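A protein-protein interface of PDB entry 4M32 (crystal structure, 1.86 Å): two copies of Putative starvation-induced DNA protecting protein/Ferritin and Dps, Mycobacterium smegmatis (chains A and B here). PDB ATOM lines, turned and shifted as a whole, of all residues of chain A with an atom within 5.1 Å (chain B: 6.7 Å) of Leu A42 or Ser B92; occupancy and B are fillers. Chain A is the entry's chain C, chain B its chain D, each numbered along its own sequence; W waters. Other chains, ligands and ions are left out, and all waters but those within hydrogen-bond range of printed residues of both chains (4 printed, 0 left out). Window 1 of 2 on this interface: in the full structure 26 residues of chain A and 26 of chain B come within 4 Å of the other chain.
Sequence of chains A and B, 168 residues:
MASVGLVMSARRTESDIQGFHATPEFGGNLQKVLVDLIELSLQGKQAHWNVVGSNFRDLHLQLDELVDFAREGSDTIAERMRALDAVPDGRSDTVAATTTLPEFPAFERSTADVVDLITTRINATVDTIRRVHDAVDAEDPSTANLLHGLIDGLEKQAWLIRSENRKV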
ATOM      1  N   ILE A  38      21.842  -1.136  23.510  1.00  0.00           N
ATOM      2  CA  ILE A  38      22.346  -1.214  22.139  1.00  0.00           C
ATOM      3  C   ILE A  38      21.621  -2.321  21.376  1.00  0.00           C
ATOM      4  O   ILE A  38      21.183  -2.109  20.245  1.00  0.00           O
ATOM      5  CB  ILE A  38      23.882  -1.420  22.080  1.00  0.00           C
ATOM      6  CG1 ILE A  38      24.607  -0.193  22.647  1.00  0.00           C
ATOM      7  CG2 ILE A  38      24.337  -1.686  20.636  1.00  0.00           C
ATOM      8  CD1 ILE A  38      26.075  -0.416  22.963  1.00  0.00           C
ATOM      9  N   GLU A  39      21.479  -3.489  22.007  1.00  0.00           N
ATOM     10  CA  GLU A  39      20.760  -4.607  21.391  1.00  0.00           C
ATOM     11  C   GLU A  39      19.317  -4.235  21.069  1.00  0.00           C
ATOM     12  O   GLU A  39      18.818  -4.567  19.995  1.00  0.00           O
ATOM     13  CB  GLU A  39      20.805  -5.860  22.275  1.00  0.00           C
ATOM     14  CG  GLU A  39      20.025  -7.068  21.718  1.00  0.00           C
ATOM     15  CD  GLU A  39      20.641  -7.682  20.459  1.00  0.00           C
ATOM     16  OE1 GLU A  39      21.734  -7.252  20.031  1.00  0.00           O
ATOM     17  OE2 GLU A  39      20.024  -8.612  19.898  1.00  0.00           O
ATOM     18  N   LEU A  40      18.652  -3.545  21.995  1.00  0.00           N
ATOM     19  CA  LEU A  40      17.277  -3.105  21.773  1.00  0.00           C
ATOM     20  C   LEU A  40      17.177  -2.164  20.573  1.00  0.00           C
ATOM     21  O   LEU A  40      16.246  -2.273  19.772  1.00  0.00           O
ATOM     22  CB  LEU A  40      16.696  -2.441  23.031  1.00  0.00           C
ATOM     23  CG  LEU A  40      15.224  -2.007  22.978  1.00  0.00           C
ATOM     24  CD1 LEU A  40      14.277  -3.185  22.735  1.00  0.00           C
ATOM     25  CD2 LEU A  40      14.842  -1.266  24.246  1.00  0.00           C
ATOM     26  N   SER A  41      18.140  -1.250  20.451  1.00  0.00           N
ATOM     27  CA  SER A  41      18.159  -0.302  19.342  1.00  0.00           C
ATOM     28  C   SER A  41      18.371  -1.006  17.997  1.00  0.00           C
ATOM     29  O   SER A  41      17.785  -0.609  16.990  1.00  0.00           O
ATOM     30  CB  SER A  41      19.207   0.795  19.567  1.00  0.00           C
ATOM     31  OG  SER A  41      20.523   0.284  19.495  1.00  0.00           O
ATOM     32  N   LEU A  42      19.207  -2.042  17.995  1.00  0.00           N
ATOM     33  CA  LEU A  42      19.448  -2.840  16.790  1.00  0.00           C
ATOM     34  C   LEU A  42      18.220  -3.669  16.434  1.00  0.00           C
ATOM     35  O   LEU A  42      17.836  -3.750  15.267  1.00  0.00           O
ATOM     36  CB  LEU A  42      20.677  -3.737  16.958  1.00  0.00           C
ATOM     37  CG  LEU A  42      22.061  -3.081  16.992  1.00  0.00           C
ATOM     38  CD1 LEU A  42      23.105  -4.073  17.489  1.00  0.00           C
ATOM     39  CD2 LEU A  42      22.455  -2.518  15.625  1.00  0.00           C
ATOM     40  N   GLN A  43      17.605  -4.279  17.443  1.00  0.00           N
ATOM     41  CA  GLN A  43      16.378  -5.048  17.237  1.00  0.00           C
ATOM     42  C   GLN A  43      15.220  -4.143  16.814  1.00  0.00           C
ATOM     43  O   GLN A  43      14.391  -4.528  15.988  1.00  0.00           O
ATOM     44  CB  GLN A  43      16.004  -5.819  18.499  1.00  0.00           C
ATOM     45  CG  GLN A  43      16.929  -6.982  18.828  1.00  0.00           C
ATOM     46  CD  GLN A  43      16.410  -7.811  19.988  1.00  0.00           C
ATOM     47  OE1 GLN A  43      15.349  -7.520  20.539  1.00  0.00           O
ATOM     48  NE2 GLN A  43      17.158  -8.837  20.374  1.00  0.00           N
ATOM     49  N   GLY A  44      15.178  -2.939  17.381  1.00  0.00           N
ATOM     50  CA  GLY A  44      14.151  -1.955  17.048  1.00  0.00           C
ATOM     51  C   GLY A  44      14.188  -1.535  15.589  1.00  0.00           C
ATOM     52  O   GLY A  44      13.140  -1.402  14.954  1.00  0.00           O
ATOM     53  N   LYS A  45      15.393  -1.314  15.063  1.00  0.00           N
ATOM     54  CA  LYS A  45      15.567  -0.986  13.648  1.00  0.00           C
ATOM     55  C   LYS A  45      15.202  -2.164  12.753  1.00  0.00           C
ATOM     56  O   LYS A  45      14.567  -1.979  11.714  1.00  0.00           O
ATOM     57  CB  LYS A  45      16.998  -0.518  13.352  1.00  0.00           C
ATOM     58  CG  LYS A  45      17.223   0.973  13.565  1.00  0.00           C
ATOM     59  CD  LYS A  45      16.399   1.794  12.574  1.00  0.00           C
ATOM     60  CE  LYS A  45      16.555   3.282  12.804  1.00  0.00           C
ATOM     61  NZ  LYS A  45      15.824   4.044  11.753  1.00  0.00           N
ATOM     62  N   GLN A  46      15.603  -3.364  13.165  1.00  0.00           N
ATOM     63  CA  GLN A  46      15.259  -4.593  12.446  1.00  0.00           C
ATOM     64  C   GLN A  46      13.742  -4.720  12.301  1.00  0.00           C
ATOM     65  O   GLN A  46      13.241  -4.978  11.206  1.00  0.00           O
ATOM     66  CB  GLN A  46      15.841  -5.822  13.165  1.00  0.00           C
ATOM     67  CG  GLN A  46      15.562  -7.164  12.474  1.00  0.00           C
ATOM     68  CD  GLN A  46      16.444  -7.420  11.254  1.00  0.00           C
ATOM     69  OE1 GLN A  46      17.395  -6.687  10.987  1.00  0.00           O
ATOM     70  NE2 GLN A  46      16.123  -8.473  10.511  1.00  0.00           N
ATOM     71  N   SER A  92      29.999  -4.828  18.441  1.00  0.00           N
ATOM     72  CA  SER A  92      29.028  -5.817  17.965  1.00  0.00           C
ATOM     73  C   SER A  92      29.200  -7.206  18.588  1.00  0.00           C
ATOM     74  O   SER A  92      28.221  -7.807  19.027  1.00  0.00           O
ATOM     75  CB  SER A  92      29.055  -5.922  16.440  1.00  0.00           C
ATOM     76  OG  SER A  92      30.346  -6.279  15.975  1.00  0.00           O
ATOM     77  N   VAL A  95      28.168  -7.075  22.350  1.00  0.00           N
ATOM     78  CA  VAL A  95      26.714  -6.957  22.450  1.00  0.00           C
ATOM     79  C   VAL A  95      26.050  -8.315  22.189  1.00  0.00           C
ATOM     80  O   VAL A  95      25.273  -8.785  23.011  1.00  0.00           O
ATOM     81  CB  VAL A  95      26.150  -5.845  21.516  1.00  0.00           C
ATOM     82  CG1 VAL A  95      24.626  -5.844  21.521  1.00  0.00           C
ATOM     83  CG2 VAL A  95      26.681  -4.473  21.941  1.00  0.00           C
ATOM     84  N   ALA A  96      26.394  -8.954  21.071  1.00  0.00           N
ATOM     85  CA  ALA A  96      25.837 -10.264  20.721  1.00  0.00           C
ATOM     86  C   ALA A  96      26.134 -11.338  21.774  1.00  0.00           C
ATOM     87  O   ALA A  96      25.262 -12.144  22.109  1.00  0.00           O
ATOM     88  CB  ALA A  96      26.337 -10.710  19.350  1.00  0.00           C
ATOM     89  N   ILE B  38      26.428  -0.532   9.645  1.00  0.00           N
ATOM     90  CA  ILE B  38      26.045  -0.719  11.045  1.00  0.00           C
ATOM     91  C   ILE B  38      27.277  -0.946  11.915  1.00  0.00           C
ATOM     92  O   ILE B  38      27.396  -0.353  12.988  1.00  0.00           O
ATOM     93  CB  ILE B  38      25.014  -1.866  11.227  1.00  0.00           C
ATOM     94  CG1 ILE B  38      23.696  -1.498  10.534  1.00  0.00           C
ATOM     95  CG2 ILE B  38      24.775  -2.154  12.713  1.00  0.00           C
ATOM     96  CD1 ILE B  38      22.749  -2.653  10.336  1.00  0.00           C
ATOM     97  N   GLU B  39      28.195  -1.791  11.448  1.00  0.00           N
ATOM     98  CA  GLU B  39      29.442  -2.035  12.179  1.00  0.00           C
ATOM     99  C   GLU B  39      30.246  -0.748  12.365  1.00  0.00           C
ATOM    100  O   GLU B  39      30.763  -0.487  13.455  1.00  0.00           O
ATOM    101  CB  GLU B  39      30.288  -3.118  11.491  1.00  0.00           C
ATOM    102  CG  GLU B  39      31.637  -3.409  12.169  1.00  0.00           C
ATOM    103  CD  GLU B  39      31.512  -4.083  13.530  1.00  0.00           C
ATOM    104  OE1 GLU B  39      32.547  -4.215  14.216  1.00  0.00           O
ATOM    105  OE2 GLU B  39      30.395  -4.480  13.920  1.00  0.00           O
ATOM    106  N   LEU B  42      28.670   1.295  15.070  1.00  0.00           N
ATOM    107  CA  LEU B  42      28.959   0.733  16.390  1.00  0.00           C
ATOM    108  C   LEU B  42      30.394   1.010  16.838  1.00  0.00           C
ATOM    109  O   LEU B  42      30.630   1.385  17.988  1.00  0.00           O
ATOM    110  CB  LEU B  42      28.643  -0.773  16.427  1.00  0.00           C
ATOM    111  CG  LEU B  42      27.169  -1.191  16.293  1.00  0.00           C
ATOM    112  CD1 LEU B  42      27.047  -2.689  16.054  1.00  0.00           C
ATOM    113  CD2 LEU B  42      26.350  -0.780  17.511  1.00  0.00           C
ATOM    114  N   ASP B  89      19.067  -7.568   7.204  1.00  0.00           N
ATOM    115  CA  ASP B  89      19.351  -8.165   8.499  1.00  0.00           C
ATOM    116  C   ASP B  89      20.438  -7.347   9.194  1.00  0.00           C
ATOM    117  O   ASP B  89      21.628  -7.492   8.904  1.00  0.00           O
ATOM    118  CB  ASP B  89      19.765  -9.636   8.352  1.00  0.00           C
ATOM    119  CG  ASP B  89      19.987 -10.322   9.692  1.00  0.00           C
ATOM    120  OD1 ASP B  89      19.832  -9.668  10.747  1.00  0.00           O
ATOM    121  OD2 ASP B  89      20.320 -11.526   9.694  1.00  0.00           O
ATOM    122  N   GLY B  90      20.009  -6.481  10.110  1.00  0.00           N
ATOM    123  CA  GLY B  90      20.928  -5.638  10.870  1.00  0.00           C
ATOM    124  C   GLY B  90      21.095  -6.051  12.321  1.00  0.00           C
ATOM    125  O   GLY B  90      21.477  -5.233  13.162  1.00  0.00           O
ATOM    126  N   ARG B  91      20.816  -7.319  12.618  1.00  0.00           N
ATOM    127  CA  ARG B  91      20.920  -7.827  13.987  1.00  0.00           C
ATOM    128  C   ARG B  91      22.383  -7.982  14.389  1.00  0.00           C
ATOM    129  O   ARG B  91      23.238  -8.205  13.533  1.00  0.00           O
ATOM    130  CB  ARG B  91      20.176  -9.155  14.135  1.00  0.00           C
ATOM    131  CG  ARG B  91      18.675  -9.052  13.864  1.00  0.00           C
ATOM    132  CD  ARG B  91      18.018 -10.420  13.845  1.00  0.00           C
ATOM    133  NE  ARG B  91      18.610 -11.304  12.843  1.00  0.00           N
ATOM    134  CZ  ARG B  91      18.487 -12.629  12.840  1.00  0.00           C
ATOM    135  NH1 ARG B  91      17.789 -13.240  13.789  1.00  0.00           N
ATOM    136  NH2 ARG B  91      19.071 -13.346  11.886  1.00  0.00           N
ATOM    137  N   SER B  92      22.658  -7.857  15.689  1.00  0.00           N
ATOM    138  CA  SER B  92      24.032  -7.875  16.212  1.00  0.00           C
ATOM    139  C   SER B  92      24.836  -9.107  15.789  1.00  0.00           C
ATOM    140  O   SER B  92      25.963  -8.972  15.312  1.00  0.00           O
ATOM    141  CB  SER B  92      24.043  -7.737  17.737  1.00  0.00           C
ATOM    142  OG  SER B  92      23.276  -8.760  18.353  1.00  0.00           O
ATOM    143  N   ASP B  93      24.257 -10.296  15.959  1.00  0.00           N
ATOM    144  CA  ASP B  93      24.953 -11.540  15.601  1.00  0.00           C
ATOM    145  C   ASP B  93      25.370 -11.544  14.135  1.00  0.00           C
ATOM    146  O   ASP B  93      26.499 -11.905  13.809  1.00  0.00           O
ATOM    147  CB  ASP B  93      24.097 -12.776  15.907  1.00  0.00           C
ATOM    148  CG  ASP B  93      23.718 -12.873  17.364  1.00  0.00           C
ATOM    149  OD1 ASP B  93      24.392 -13.618  18.112  1.00  0.00           O
ATOM    150  OD2 ASP B  93      22.749 -12.198  17.764  1.00  0.00           O
ATOM    151  N   THR B  94      24.453 -11.129  13.264  1.00  0.00           N
ATOM    152  CA  THR B  94      24.699 -11.085  11.826  1.00  0.00           C
ATOM    153  C   THR B  94      25.771 -10.059  11.458  1.00  0.00           C
ATOM    154  O   THR B  94      26.660 -10.343  10.651  1.00  0.00           O
ATOM    155  CB  THR B  94      23.395 -10.802  11.048  1.00  0.00           C
ATOM    156  OG1 THR B  94      22.465 -11.862  11.293  1.00  0.00           O
ATOM    157  CG2 THR B  94      23.657 -10.700   9.548  1.00  0.00           C
ATOM    158  N   VAL B  95      25.687  -8.872  12.056  1.00  0.00           N
ATOM    159  CA  VAL B  95      26.673  -7.821  11.811  1.00  0.00           C
ATOM    160  C   VAL B  95      28.070  -8.301  12.227  1.00  0.00           C
ATOM    161  O   VAL B  95      29.011  -8.219  11.440  1.00  0.00           O
ATOM    162  CB  VAL B  95      26.287  -6.484  12.508  1.00  0.00           C
ATOM    163  CG1 VAL B  95      27.426  -5.476  12.426  1.00  0.00           C
ATOM    164  CG2 VAL B  95      25.014  -5.904  11.883  1.00  0.00           C
ATOM    165  N   ALA B  96      28.183  -8.833  13.441  1.00  0.00           N
ATOM    166  CA  ALA B  96      29.452  -9.363  13.949  1.00  0.00           C
ATOM    167  C   ALA B  96      30.006 -10.503  13.087  1.00  0.00           C
ATOM    168  O   ALA B  96      31.211 -10.562  12.830  1.00  0.00           O
ATOM    169  CB  ALA B  96      29.301  -9.813  15.391  1.00  0.00           C
ATOM    170  N   ALA B  97      29.120 -11.389  12.635  1.00  0.00           N
ATOM    171  CA  ALA B  97      29.519 -12.570  11.863  1.00  0.00           C
ATOM    172  C   ALA B  97      29.890 -12.275  10.410  1.00  0.00           C
ATOM    173  O   ALA B  97      30.667 -13.020   9.806  1.00  0.00           O
ATOM    174  CB  ALA B  97      28.433 -13.638  11.922  1.00  0.00           C
HETATM  175  O   HOH W   1      19.810  -3.079  13.260  1.00  0.00           O
HETATM  176  O   HOH W   2      23.680 -13.881  20.621  1.00  0.00           O
HETATM  177  O   HOH W   3      20.119  -7.304  17.148  1.00  0.00           O
HETATM  178  O   HOH W   4      31.641  -3.116  16.675  1.00  0.00           O
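OE1 of Gln A46 sits at hydrogen-bond distance from N of Gly B90 (2.8 Å).
OE2 of Glu B39 lies within hydrogen-bond range of OG of Ser A92, at 2.7 Å.
The side-chain carboxylate (OE1) of Glu A39 sits at hydrogen-bond distance from the side-chain hydroxyl (OG) of Ser B92, at 2.7 Å.
The side-chain carboxylate of Glu A39 is in hydrogen-bond range of the side-chain amide nitrogen of Gln A43, at 2.9 Å.
O of Ile A38 is in hydrogen-bond range of OG of Ser A41 (2.6 Å).
OD1 of Asp B89 lies within salt-bridge range of NE of Arg B91, at 2.9 Å.
The side-chain carboxylate of Asp B89 lies within hydrogen-bond range of the side-chain hydroxyl of Thr B94, 2.7 Å away.
Ile A38 touches Leu B42, and with the chains exchanged Leu A42 touches Ile B38.
Glu A39 touches Ser B92, and with the chains exchanged Ser A92 touches Glu B39.
Leu A42 touches Ser B92, and with the chains exchanged Ser A92 touches Leu B42.
Ser A92 touches Ala B96, and with the chains exchanged Ala A96 touches Ser B92.
Of the 13 pairs that touch across the chains among the printed residues, 8 have their exchanged pair printed and touching as well.
Ser A41 touches none of the printed residues of chain B.
Printed residues of chain B within 4 Å of Leu A42: Ile B38, Gly B90 and Ser B92.
Of chain A, only Glu A39, Leu A42 and Ala A96 come within 4 Å of Ser B92.
Of the printed residues of chain A, Asp B93 touches Ala A96.
Thr B94 touches none of the printed residues of chain A.
Of the printed residues of chain A, Ala B96 touches Ser A92 (3.7 Å).
The nearest residue of chain B that does not touch Leu A42 is Leu B42 (4.4 Å).
The nearest residue of chain A that does not touch Ser B92 is Val A95 (4.3 Å).
The nearest printed residue of chain A that does not touch Glu B39 is Leu A42 (7.1 Å).
Water W2 lies within hydrogen-bond range of the side-chain carboxylate of Asp B93 (2.6 Å) and the backbone carbonyl oxygen of Ala A96 (2.8 Å).
Water W1 bridges the backbone carbonyl oxygen (O) of Gly B90 and the backbone carbonyl oxygen (O) of Leu A42.
Water W4 lies within hydrogen-bond range of the side-chain carboxylate of Glu B39 (2.8 Å) and the backbone NH of Ser A92 (3.0 Å).
Water W3 bridges the backbone NH (N) of Ser B92 (3.0 Å) and the side-chain carboxylate (OE2) of Glu A39 (3.0 Å).
Among the printed residues, merely in contact across the chains: Gln A46 with Asp B89, Ala A96 with Asp B93, Ser A92 with Ala B96, Leu A42 with Ile B38, Ala A96 with Ser B92, Leu A42 with Ser B92, Leu A42 with Gly B90, Gln A46 with Arg B91, Ser A92 with Leu B42 and Ile A38 with Leu B42.
Of the 12 printed residues of chain B, 9 touch a printed residue of chain A.
Printed residues of chain B that touch a printed residue of chain A: Ile B38, Glu B39, Leu B42, Asp B89, Gly B90, Arg B91, Ser B92, Asp B93 and Ala B96.
Of the 12 printed residues of chain A, 6 touch a printed residue of chain B.
Printed residues of chain A that touch a printed residue of chain B: Ile A38, Glu A39, Leu A42, Gln A46, Ser A92 and Ala A96.
Hydrophobic or aromatic side chains of chain A that line the printed part of chain B: Ile A38, Leu A42 and Ala A96.
Among the printed residues, no Asp or Glu carboxylate lies within 4 Å of a Lys or Arg side-chain nitrogen of the other chain.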
